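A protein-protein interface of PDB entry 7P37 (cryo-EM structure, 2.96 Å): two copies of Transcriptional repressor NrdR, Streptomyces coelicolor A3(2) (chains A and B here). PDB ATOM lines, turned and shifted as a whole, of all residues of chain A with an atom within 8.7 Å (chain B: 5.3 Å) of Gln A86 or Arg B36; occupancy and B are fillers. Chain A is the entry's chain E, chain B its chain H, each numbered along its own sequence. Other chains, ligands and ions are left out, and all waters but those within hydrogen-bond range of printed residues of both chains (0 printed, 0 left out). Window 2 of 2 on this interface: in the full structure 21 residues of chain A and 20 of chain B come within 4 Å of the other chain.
The guanidinium group (NE) of Arg B36 is in hydrogen-bond range of the side-chain amide oxygen (OE1) of Gln A86 (3.2 Å).
NH1 of Arg B36 sits close to OE1 of Glu A90 (2.4 Å).
NH1 of Arg A60 is in salt-bridge range of OE1 of Glu A89, 2.5 Å away.
The guanidinium group (NE) of Arg A60 lies close to the side-chain amide nitrogen (NE2) of Gln A86 (3.1 Å).
The side-chain carboxylate (OE2) of Glu A89 is in salt-bridge range of the guanidinium group (NE) of Arg A93, 3.7 Å away.
N of Phe B5 lies close to SG of Cys B3 (3.3 Å).
The side-chain sulfur (SG) of Cys B34 lies close to the backbone NH (N) of Arg B36 (3.6 Å).
N of Cys B31 is in hydrogen-bond range of O of Arg B36.
Arg A60 touches Phe B5.
Phe B5 touches Gln A86.
Glu A89 touches Phe B5.
Phe B5 touches Glu A90.
OE2 of Glu A90 touches N of Arg B37, at 3.6 Å.
Printed residues of chain B within 4 Å of Arg A60: Phe B5 (3.7 Å).
Asp A79 touches none of the printed residues of chain B.
Printed residues of chain B within 4 Å of Glu A90: Phe B5 (3.96 Å), Arg B36 (2.4 Å) and Arg B37 (3.6 Å).
Ala A91 touches none of the printed residues of chain B.
Printed residues of chain A within 4 Å of Phe B5: Arg A60, Gln A86, Glu A89 and Glu A90.
Of the printed residues of chain A, Arg B37 touches Glu A90 (3.6 Å).
The nearest printed residue of chain B that does not touch Gln A86 is Cys B34 (5.7 Å).
The nearest residue of chain A that does not touch Arg B36 is Arg A87 (4.4 Å).
The nearest printed residue of chain A that does not touch Arg B37 is Arg A93 (5.3 Å).
Of the 21 printed residues of chain A, 4 touch a printed residue of chain B.
Printed residues of chain A that touch a printed residue of chain B: Arg A60, Gln A86, Glu A89 and Glu A90.
Printed residues of chain B that touch a printed residue of chain A: Phe B5, Arg B36 and Arg B37.
Hydrophobic or aromatic side chains of chain B that line the printed part of chain A: Phe B5.
Among the printed residues, Asp or Glu carboxylates within 4 Å of a Lys or Arg side-chain nitrogen of the other chain: Glu A90 with Arg B36 (2.4 Å).
No position is printed for both chains.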
ATOM      1  N   PHE A  58     -16.654  26.389 -11.851  1.00  0.00           N
ATOM      2  CA  PHE A  58     -16.254  26.319 -13.249  1.00  0.00           C
ATOM      3  C   PHE A  58     -15.865  27.700 -13.760  1.00  0.00           C
ATOM      4  O   PHE A  58     -16.519  28.701 -13.454  1.00  0.00           O
ATOM      5  CB  PHE A  58     -17.391  25.742 -14.093  1.00  0.00           C
ATOM      6  CG  PHE A  58     -17.028  25.512 -15.533  1.00  0.00           C
ATOM      7  CD1 PHE A  58     -17.219  26.504 -16.481  1.00  0.00           C
ATOM      8  CD2 PHE A  58     -16.504  24.300 -15.942  1.00  0.00           C
ATOM      9  CE1 PHE A  58     -16.888  26.292 -17.804  1.00  0.00           C
ATOM     10  CE2 PHE A  58     -16.172  24.081 -17.266  1.00  0.00           C
ATOM     11  CZ  PHE A  58     -16.363  25.080 -18.196  1.00  0.00           C
ATOM     12  N   ARG A  60     -14.550  29.699 -17.400  1.00  0.00           N
ATOM     13  CA  ARG A  60     -14.271  29.680 -18.832  1.00  0.00           C
ATOM     14  C   ARG A  60     -12.880  30.218 -19.142  1.00  0.00           C
ATOM     15  O   ARG A  60     -12.270  29.820 -20.144  1.00  0.00           O
ATOM     16  CB  ARG A  60     -15.330  30.492 -19.574  1.00  0.00           C
ATOM     17  CG  ARG A  60     -15.535  30.097 -21.020  1.00  0.00           C
ATOM     18  CD  ARG A  60     -16.850  30.644 -21.554  1.00  0.00           C
ATOM     19  NE  ARG A  60     -16.944  32.095 -21.419  1.00  0.00           N
ATOM     20  CZ  ARG A  60     -17.696  32.717 -20.523  1.00  0.00           C
ATOM     21  NH1 ARG A  60     -18.440  32.047 -19.658  1.00  0.00           N
ATOM     22  NH2 ARG A  60     -17.704  34.047 -20.493  1.00  0.00           N
ATOM     23  N   THR A  61     -12.368  31.114 -18.293  1.00  0.00           N
ATOM     24  CA  THR A  61     -11.045  31.688 -18.516  1.00  0.00           C
ATOM     25  C   THR A  61      -9.962  30.618 -18.461  1.00  0.00           C
ATOM     26  O   THR A  61      -9.021  30.637 -19.261  1.00  0.00           O
ATOM     27  CB  THR A  61     -10.770  32.780 -17.482  1.00  0.00           C
ATOM     28  OG1 THR A  61     -11.814  33.760 -17.533  1.00  0.00           O
ATOM     29  CG2 THR A  61      -9.437  33.456 -17.760  1.00  0.00           C
ATOM     30  N   VAL A  63     -10.311  27.399 -19.145  1.00  0.00           N
ATOM     31  CA  VAL A  63     -10.424  26.597 -20.361  1.00  0.00           C
ATOM     32  C   VAL A  63      -9.781  27.321 -21.537  1.00  0.00           C
ATOM     33  O   VAL A  63      -9.052  26.718 -22.338  1.00  0.00           O
ATOM     34  CB  VAL A  63     -11.901  26.262 -20.640  1.00  0.00           C
ATOM     35  CG1 VAL A  63     -12.057  25.633 -22.013  1.00  0.00           C
ATOM     36  CG2 VAL A  63     -12.449  25.343 -19.561  1.00  0.00           C
ATOM     37  N   ILE A  64     -10.042  28.626 -21.657  1.00  0.00           N
ATOM     38  CA  ILE A  64      -9.459  29.407 -22.744  1.00  0.00           C
ATOM     39  C   ILE A  64      -7.941  29.427 -22.634  1.00  0.00           C
ATOM     40  O   ILE A  64      -7.231  29.274 -23.633  1.00  0.00           O
ATOM     41  CB  ILE A  64     -10.051  30.828 -22.756  1.00  0.00           C
ATOM     42  CG1 ILE A  64     -11.533  30.782 -23.129  1.00  0.00           C
ATOM     43  CG2 ILE A  64      -9.289  31.719 -23.721  1.00  0.00           C
ATOM     44  CD1 ILE A  64     -12.219  32.127 -23.067  1.00  0.00           C
ATOM     45  N   ASP A  79     -10.996  35.522 -30.807  1.00  0.00           N
ATOM     46  CA  ASP A  79     -12.428  35.300 -30.982  1.00  0.00           C
ATOM     47  C   ASP A  79     -12.744  33.812 -31.068  1.00  0.00           C
ATOM     48  O   ASP A  79     -13.726  33.341 -30.482  1.00  0.00           O
ATOM     49  CB  ASP A  79     -12.926  36.027 -32.231  1.00  0.00           C
ATOM     50  CG  ASP A  79     -12.999  37.529 -32.040  1.00  0.00           C
ATOM     51  OD1 ASP A  79     -12.609  38.014 -30.957  1.00  0.00           O
ATOM     52  OD2 ASP A  79     -13.447  38.227 -32.974  1.00  0.00           O
ATOM     53  N   ALA A  80     -11.917  33.055 -31.794  1.00  0.00           N
ATOM     54  CA  ALA A  80     -12.118  31.614 -31.887  1.00  0.00           C
ATOM     55  C   ALA A  80     -11.960  30.944 -30.527  1.00  0.00           C
ATOM     56  O   ALA A  80     -12.726  30.039 -30.181  1.00  0.00           O
ATOM     57  CB  ALA A  80     -11.146  31.011 -32.898  1.00  0.00           C
ATOM     58  N   LEU A  81     -10.968  31.373 -29.744  1.00  0.00           N
ATOM     59  CA  LEU A  81     -10.779  30.801 -28.416  1.00  0.00           C
ATOM     60  C   LEU A  81     -11.955  31.118 -27.499  1.00  0.00           C
ATOM     61  O   LEU A  81     -12.405  30.256 -26.735  1.00  0.00           O
ATOM     62  CB  LEU A  81      -9.471  31.306 -27.808  1.00  0.00           C
ATOM     63  CG  LEU A  81      -8.190  30.813 -28.484  1.00  0.00           C
ATOM     64  CD1 LEU A  81      -6.968  31.315 -27.736  1.00  0.00           C
ATOM     65  CD2 LEU A  81      -8.178  29.298 -28.582  1.00  0.00           C
ATOM     66  N   ALA A  82     -12.464  32.352 -27.559  1.00  0.00           N
ATOM     67  CA  ALA A  82     -13.626  32.709 -26.750  1.00  0.00           C
ATOM     68  C   ALA A  82     -14.849  31.895 -27.152  1.00  0.00           C
ATOM     69  O   ALA A  82     -15.607  31.432 -26.291  1.00  0.00           O
ATOM     70  CB  ALA A  82     -13.909  34.205 -26.871  1.00  0.00           C
ATOM     71  N   GLN A  83     -15.055  31.708 -28.456  1.00  0.00           N
ATOM     72  CA  GLN A  83     -16.182  30.901 -28.914  1.00  0.00           C
ATOM     73  C   GLN A  83     -16.032  29.446 -28.479  1.00  0.00           C
ATOM     74  O   GLN A  83     -17.020  28.802 -28.106  1.00  0.00           O
ATOM     75  CB  GLN A  83     -16.315  30.999 -30.432  1.00  0.00           C
ATOM     76  CG  GLN A  83     -17.587  30.381 -30.979  1.00  0.00           C
ATOM     77  CD  GLN A  83     -17.863  30.791 -32.409  1.00  0.00           C
ATOM     78  OE1 GLN A  83     -17.009  31.381 -33.072  1.00  0.00           O
ATOM     79  NE2 GLN A  83     -19.061  30.484 -32.893  1.00  0.00           N
ATOM     80  N   LEU A  84     -14.811  28.911 -28.529  1.00  0.00           N
ATOM     81  CA  LEU A  84     -14.581  27.548 -28.059  1.00  0.00           C
ATOM     82  C   LEU A  84     -14.873  27.424 -26.570  1.00  0.00           C
ATOM     83  O   LEU A  84     -15.468  26.434 -26.129  1.00  0.00           O
ATOM     84  CB  LEU A  84     -13.145  27.120 -28.372  1.00  0.00           C
ATOM     85  CG  LEU A  84     -12.738  25.662 -28.126  1.00  0.00           C
ATOM     86  CD1 LEU A  84     -11.652  25.258 -29.099  1.00  0.00           C
ATOM     87  CD2 LEU A  84     -12.244  25.454 -26.701  1.00  0.00           C
ATOM     88  N   GLY A  85     -14.458  28.414 -25.780  1.00  0.00           N
ATOM     89  CA  GLY A  85     -14.776  28.388 -24.360  1.00  0.00           C
ATOM     90  C   GLY A  85     -16.269  28.438 -24.102  1.00  0.00           C
ATOM     91  O   GLY A  85     -16.786  27.725 -23.234  1.00  0.00           O
ATOM     92  N   GLN A  86     -16.984  29.279 -24.855  1.00  0.00           N
ATOM     93  CA  GLN A  86     -18.438  29.342 -24.721  1.00  0.00           C
ATOM     94  C   GLN A  86     -19.080  28.005 -25.066  1.00  0.00           C
ATOM     95  O   GLN A  86     -19.987  27.542 -24.364  1.00  0.00           O
ATOM     96  CB  GLN A  86     -18.998  30.448 -25.613  1.00  0.00           C
ATOM     97  CG  GLN A  86     -18.646  31.856 -25.167  1.00  0.00           C
ATOM     98  CD  GLN A  86     -19.713  32.472 -24.288  1.00  0.00           C
ATOM     99  OE1 GLN A  86     -20.896  32.456 -24.625  1.00  0.00           O
ATOM    100  NE2 GLN A  86     -19.300  33.022 -23.155  1.00  0.00           N
ATOM    101  N   ARG A  87     -18.622  27.371 -26.150  1.00  0.00           N
ATOM    102  CA  ARG A  87     -19.168  26.075 -26.540  1.00  0.00           C
ATOM    103  C   ARG A  87     -18.894  25.018 -25.479  1.00  0.00           C
ATOM    104  O   ARG A  87     -19.768  24.199 -25.168  1.00  0.00           O
ATOM    105  CB  ARG A  87     -18.585  25.642 -27.884  1.00  0.00           C
ATOM    106  CG  ARG A  87     -19.066  26.461 -29.065  1.00  0.00           C
ATOM    107  CD  ARG A  87     -18.493  25.926 -30.366  1.00  0.00           C
ATOM    108  NE  ARG A  87     -18.658  24.481 -30.476  1.00  0.00           N
ATOM    109  CZ  ARG A  87     -18.236  23.756 -31.503  1.00  0.00           C
ATOM    110  NH1 ARG A  87     -17.614  24.308 -32.532  1.00  0.00           N
ATOM    111  NH2 ARG A  87     -18.443  22.443 -31.497  1.00  0.00           N
ATOM    112  N   VAL A  88     -17.685  25.018 -24.914  1.00  0.00           N
ATOM    113  CA  VAL A  88     -17.343  24.046 -23.880  1.00  0.00           C
ATOM    114  C   VAL A  88     -18.228  24.241 -22.655  1.00  0.00           C
ATOM    115  O   VAL A  88     -18.758  23.277 -22.090  1.00  0.00           O
ATOM    116  CB  VAL A  88     -15.850  24.149 -23.520  1.00  0.00           C
ATOM    117  CG1 VAL A  88     -15.565  23.448 -22.202  1.00  0.00           C
ATOM    118  CG2 VAL A  88     -14.998  23.560 -24.631  1.00  0.00           C
ATOM    119  N   GLU A  89     -18.408  25.496 -22.231  1.00  0.00           N
ATOM    120  CA  GLU A  89     -19.246  25.761 -21.065  1.00  0.00           C
ATOM    121  C   GLU A  89     -20.693  25.357 -21.317  1.00  0.00           C
ATOM    122  O   GLU A  89     -21.344  24.776 -20.440  1.00  0.00           O
ATOM    123  CB  GLU A  89     -19.163  27.235 -20.674  1.00  0.00           C
ATOM    124  CG  GLU A  89     -19.837  27.551 -19.349  1.00  0.00           C
ATOM    125  CD  GLU A  89     -19.759  29.019 -18.987  1.00  0.00           C
ATOM    126  OE1 GLU A  89     -19.559  29.848 -19.898  1.00  0.00           O
ATOM    127  OE2 GLU A  89     -19.898  29.348 -17.790  1.00  0.00           O
ATOM    128  N   GLU A  90     -21.217  25.652 -22.509  1.00  0.00           N
ATOM    129  CA  GLU A  90     -22.593  25.276 -22.817  1.00  0.00           C
ATOM    130  C   GLU A  90     -22.764  23.763 -22.842  1.00  0.00           C
ATOM    131  O   GLU A  90     -23.748  23.232 -22.312  1.00  0.00           O
ATOM    132  CB  GLU A  90     -23.021  25.886 -24.152  1.00  0.00           C
ATOM    133  CG  GLU A  90     -24.488  25.680 -24.479  1.00  0.00           C
ATOM    134  CD  GLU A  90     -24.910  26.392 -25.747  1.00  0.00           C
ATOM    135  OE1 GLU A  90     -24.032  26.949 -26.436  1.00  0.00           O
ATOM    136  OE2 GLU A  90     -26.121  26.396 -26.054  1.00  0.00           O
ATOM    137  N   ALA A  91     -21.813  23.046 -23.450  1.00  0.00           N
ATOM    138  CA  ALA A  91     -21.909  21.593 -23.513  1.00  0.00           C
ATOM    139  C   ALA A  91     -21.792  20.968 -22.128  1.00  0.00           C
ATOM    140  O   ALA A  91     -22.469  19.978 -21.830  1.00  0.00           O
ATOM    141  CB  ALA A  91     -20.837  21.034 -24.447  1.00  0.00           C
ATOM    142  N   VAL A  92     -20.933  21.526 -21.275  1.00  0.00           N
ATOM    143  CA  VAL A  92     -20.793  21.007 -19.918  1.00  0.00           C
ATOM    144  C   VAL A  92     -22.080  21.212 -19.128  1.00  0.00           C
ATOM    145  O   VAL A  92     -22.552  20.303 -18.438  1.00  0.00           O
ATOM    146  CB  VAL A  92     -19.585  21.660 -19.223  1.00  0.00           C
ATOM    147  CG1 VAL A  92     -19.686  21.496 -17.723  1.00  0.00           C
ATOM    148  CG2 VAL A  92     -18.292  21.051 -19.736  1.00  0.00           C
ATOM    149  N   ARG A  93     -22.673  22.405 -19.222  1.00  0.00           N
ATOM    150  CA  ARG A  93     -23.893  22.686 -18.474  1.00  0.00           C
ATOM    151  C   ARG A  93     -25.088  21.901 -19.002  1.00  0.00           C
ATOM    152  O   ARG A  93     -26.048  21.677 -18.256  1.00  0.00           O
ATOM    153  CB  ARG A  93     -24.199  24.183 -18.504  1.00  0.00           C
ATOM    154  CG  ARG A  93     -23.195  25.036 -17.753  1.00  0.00           C
ATOM    155  CD  ARG A  93     -23.647  26.483 -17.675  1.00  0.00           C
ATOM    156  NE  ARG A  93     -22.764  27.285 -16.837  1.00  0.00           N
ATOM    157  CZ  ARG A  93     -22.924  27.458 -15.533  1.00  0.00           C
ATOM    158  NH1 ARG A  93     -23.928  26.897 -14.879  1.00  0.00           N
ATOM    159  NH2 ARG A  93     -22.056  28.212 -14.867  1.00  0.00           N
ATOM    160  N   PRO A 112     -14.695  20.620 -29.942  1.00  0.00           N
ATOM    161  CA  PRO A 112     -14.414  21.842 -30.713  1.00  0.00           C
ATOM    162  C   PRO A 112     -12.949  22.020 -31.073  1.00  0.00           C
ATOM    163  O   PRO A 112     -12.644  22.637 -32.102  1.00  0.00           O
ATOM    164  CB  PRO A 112     -14.903  22.962 -29.783  1.00  0.00           C
ATOM    165  CG  PRO A 112     -15.866  22.302 -28.856  1.00  0.00           C
ATOM    166  CD  PRO A 112     -15.346  20.916 -28.655  1.00  0.00           C
ATOM    167  N   CYS B   3     -27.821  35.336 -16.931  1.00  0.00           N
ATOM    168  CA  CYS B   3     -27.226  34.345 -17.815  1.00  0.00           C
ATOM    169  C   CYS B   3     -25.791  34.056 -17.384  1.00  0.00           C
ATOM    170  O   CYS B   3     -25.033  34.992 -17.104  1.00  0.00           O
ATOM    171  CB  CYS B   3     -27.258  34.839 -19.258  1.00  0.00           C
ATOM    172  SG  CYS B   3     -26.356  33.809 -20.427  1.00  0.00           S
ATOM    173  N   PHE B   5     -23.340  33.113 -19.177  1.00  0.00           N
ATOM    174  CA  PHE B   5     -22.379  33.433 -20.228  1.00  0.00           C
ATOM    175  C   PHE B   5     -22.184  34.939 -20.386  1.00  0.00           C
ATOM    176  O   PHE B   5     -21.070  35.447 -20.219  1.00  0.00           O
ATOM    177  CB  PHE B   5     -22.829  32.806 -21.553  1.00  0.00           C
ATOM    178  CG  PHE B   5     -23.258  31.371 -21.433  1.00  0.00           C
ATOM    179  CD1 PHE B   5     -22.324  30.370 -21.235  1.00  0.00           C
ATOM    180  CD2 PHE B   5     -24.594  31.023 -21.522  1.00  0.00           C
ATOM    181  CE1 PHE B   5     -22.716  29.049 -21.125  1.00  0.00           C
ATOM    182  CE2 PHE B   5     -24.990  29.704 -21.413  1.00  0.00           C
ATOM    183  CZ  PHE B   5     -24.050  28.715 -21.215  1.00  0.00           C
ATOM    184  N   ARG B  29     -33.465  26.670 -19.213  1.00  0.00           N
ATOM    185  CA  ARG B  29     -33.640  28.090 -19.465  1.00  0.00           C
ATOM    186  C   ARG B  29     -32.808  28.507 -20.669  1.00  0.00           C
ATOM    187  O   ARG B  29     -31.815  27.862 -21.015  1.00  0.00           O
ATOM    188  CB  ARG B  29     -33.225  28.920 -18.244  1.00  0.00           C
ATOM    189  CG  ARG B  29     -33.999  28.607 -16.980  1.00  0.00           C
ATOM    190  CD  ARG B  29     -33.503  29.449 -15.820  1.00  0.00           C
ATOM    191  NE  ARG B  29     -34.436  29.443 -14.700  1.00  0.00           N
ATOM    192  CZ  ARG B  29     -35.337  30.387 -14.473  1.00  0.00           C
ATOM    193  NH1 ARG B  29     -35.452  31.439 -15.266  1.00  0.00           N
ATOM    194  NH2 ARG B  29     -36.145  30.275 -13.423  1.00  0.00           N
ATOM    195  N   GLN B  30     -33.222  29.602 -21.305  1.00  0.00           N
ATOM    196  CA  GLN B  30     -32.497  30.165 -22.436  1.00  0.00           C
ATOM    197  C   GLN B  30     -32.382  31.670 -22.267  1.00  0.00           C
ATOM    198  O   GLN B  30     -33.352  32.337 -21.900  1.00  0.00           O
ATOM    199  CB  GLN B  30     -33.190  29.844 -23.765  1.00  0.00           C
ATOM    200  CG  GLN B  30     -32.428  30.311 -24.990  1.00  0.00           C
ATOM    201  CD  GLN B  30     -33.130  29.947 -26.282  1.00  0.00           C
ATOM    202  OE1 GLN B  30     -34.332  29.686 -26.295  1.00  0.00           O
ATOM    203  NE2 GLN B  30     -32.380  29.925 -27.376  1.00  0.00           N
ATOM    204  N   CYS B  31     -31.198  32.199 -22.540  1.00  0.00           N
ATOM    205  CA  CYS B  31     -30.981  33.638 -22.459  1.00  0.00           C
ATOM    206  C   CYS B  31     -31.570  34.324 -23.688  1.00  0.00           C
ATOM    207  O   CYS B  31     -31.297  33.902 -24.815  1.00  0.00           O
ATOM    208  CB  CYS B  31     -29.495  33.953 -22.349  1.00  0.00           C
ATOM    209  SG  CYS B  31     -29.133  35.713 -22.223  1.00  0.00           S
ATOM    210  N   CYS B  34     -28.147  36.070 -25.919  1.00  0.00           N
ATOM    211  CA  CYS B  34     -27.198  35.205 -26.607  1.00  0.00           C
ATOM    212  C   CYS B  34     -27.810  33.900 -27.100  1.00  0.00           C
ATOM    213  O   CYS B  34     -27.148  33.173 -27.847  1.00  0.00           O
ATOM    214  CB  CYS B  34     -26.013  34.891 -25.691  1.00  0.00           C
ATOM    215  SG  CYS B  34     -26.439  33.920 -24.232  1.00  0.00           S
ATOM    216  N   SER B  35     -29.048  33.591 -26.705  1.00  0.00           N
ATOM    217  CA  SER B  35     -29.740  32.374 -27.133  1.00  0.00           C
ATOM    218  C   SER B  35     -28.939  31.118 -26.792  1.00  0.00           C
ATOM    219  O   SER B  35     -28.895  30.160 -27.565  1.00  0.00           O
ATOM    220  CB  SER B  35     -30.067  32.421 -28.627  1.00  0.00           C
ATOM    221  OG  SER B  35     -30.953  33.487 -28.920  1.00  0.00           O
ATOM    222  N   ARG B  36     -28.305  31.121 -25.624  1.00  0.00           N
ATOM    223  CA  ARG B  36     -27.552  29.975 -25.126  1.00  0.00           C
ATOM    224  C   ARG B  36     -28.287  29.400 -23.923  1.00  0.00           C
ATOM    225  O   ARG B  36     -28.573  30.124 -22.963  1.00  0.00           O
ATOM    226  CB  ARG B  36     -26.125  30.372 -24.749  1.00  0.00           C
ATOM    227  CG  ARG B  36     -25.203  30.570 -25.938  1.00  0.00           C
ATOM    228  CD  ARG B  36     -23.750  30.667 -25.504  1.00  0.00           C
ATOM    229  NE  ARG B  36     -22.862  30.925 -26.631  1.00  0.00           N
ATOM    230  CZ  ARG B  36     -22.379  29.988 -27.436  1.00  0.00           C
ATOM    231  NH1 ARG B  36     -22.679  28.710 -27.268  1.00  0.00           N
ATOM    232  NH2 ARG B  36     -21.577  30.342 -28.435  1.00  0.00           N
ATOM    233  N   ARG B  37     -28.582  28.105 -23.975  1.00  0.00           N
ATOM    234  CA  ARG B  37     -29.396  27.460 -22.957  1.00  0.00           C
ATOM    235  C   ARG B  37     -28.537  26.898 -21.833  1.00  0.00           C
ATOM    236  O   ARG B  37     -27.369  26.550 -22.023  1.00  0.00           O
ATOM    237  CB  ARG B  37     -30.236  26.340 -23.573  1.00  0.00           C
ATOM    238  CG  ARG B  37     -31.160  26.806 -24.685  1.00  0.00           C
ATOM    239  CD  ARG B  37     -32.151  25.722 -25.071  1.00  0.00           C
ATOM    240  NE  ARG B  37     -33.154  26.213 -26.008  1.00  0.00           N
ATOM    241  CZ  ARG B  37     -34.222  25.526 -26.390  1.00  0.00           C
ATOM    242  NH1 ARG B  37     -34.460  24.307 -25.934  1.00  0.00           N
ATOM    243  NH2 ARG B  37     -35.074  26.076 -27.251  1.00  0.00           N
ATOM    244  N   PHE B  38     -29.137  26.816 -20.648  1.00  0.00           N
ATOM    245  CA  PHE B  38     -28.510  26.203 -19.487  1.00  0.00           C
ATOM    246  C   PHE B  38     -29.600  25.565 -18.634  1.00  0.00           C
ATOM    247  O   PHE B  38     -30.783  25.589 -18.984  1.00  0.00           O
ATOM    248  CB  PHE B  38     -27.668  27.218 -18.697  1.00  0.00           C
ATOM    249  CG  PHE B  38     -28.443  28.404 -18.188  1.00  0.00           C
ATOM    250  CD1 PHE B  38     -28.885  29.392 -19.054  1.00  0.00           C
ATOM    251  CD2 PHE B  38     -28.706  28.543 -16.837  1.00  0.00           C
ATOM    252  CE1 PHE B  38     -29.587  30.483 -18.582  1.00  0.00           C
ATOM    253  CE2 PHE B  38     -29.407  29.633 -16.361  1.00  0.00           C
ATOM    254  CZ  PHE B  38     -29.848  30.603 -17.234  1.00  0.00           C
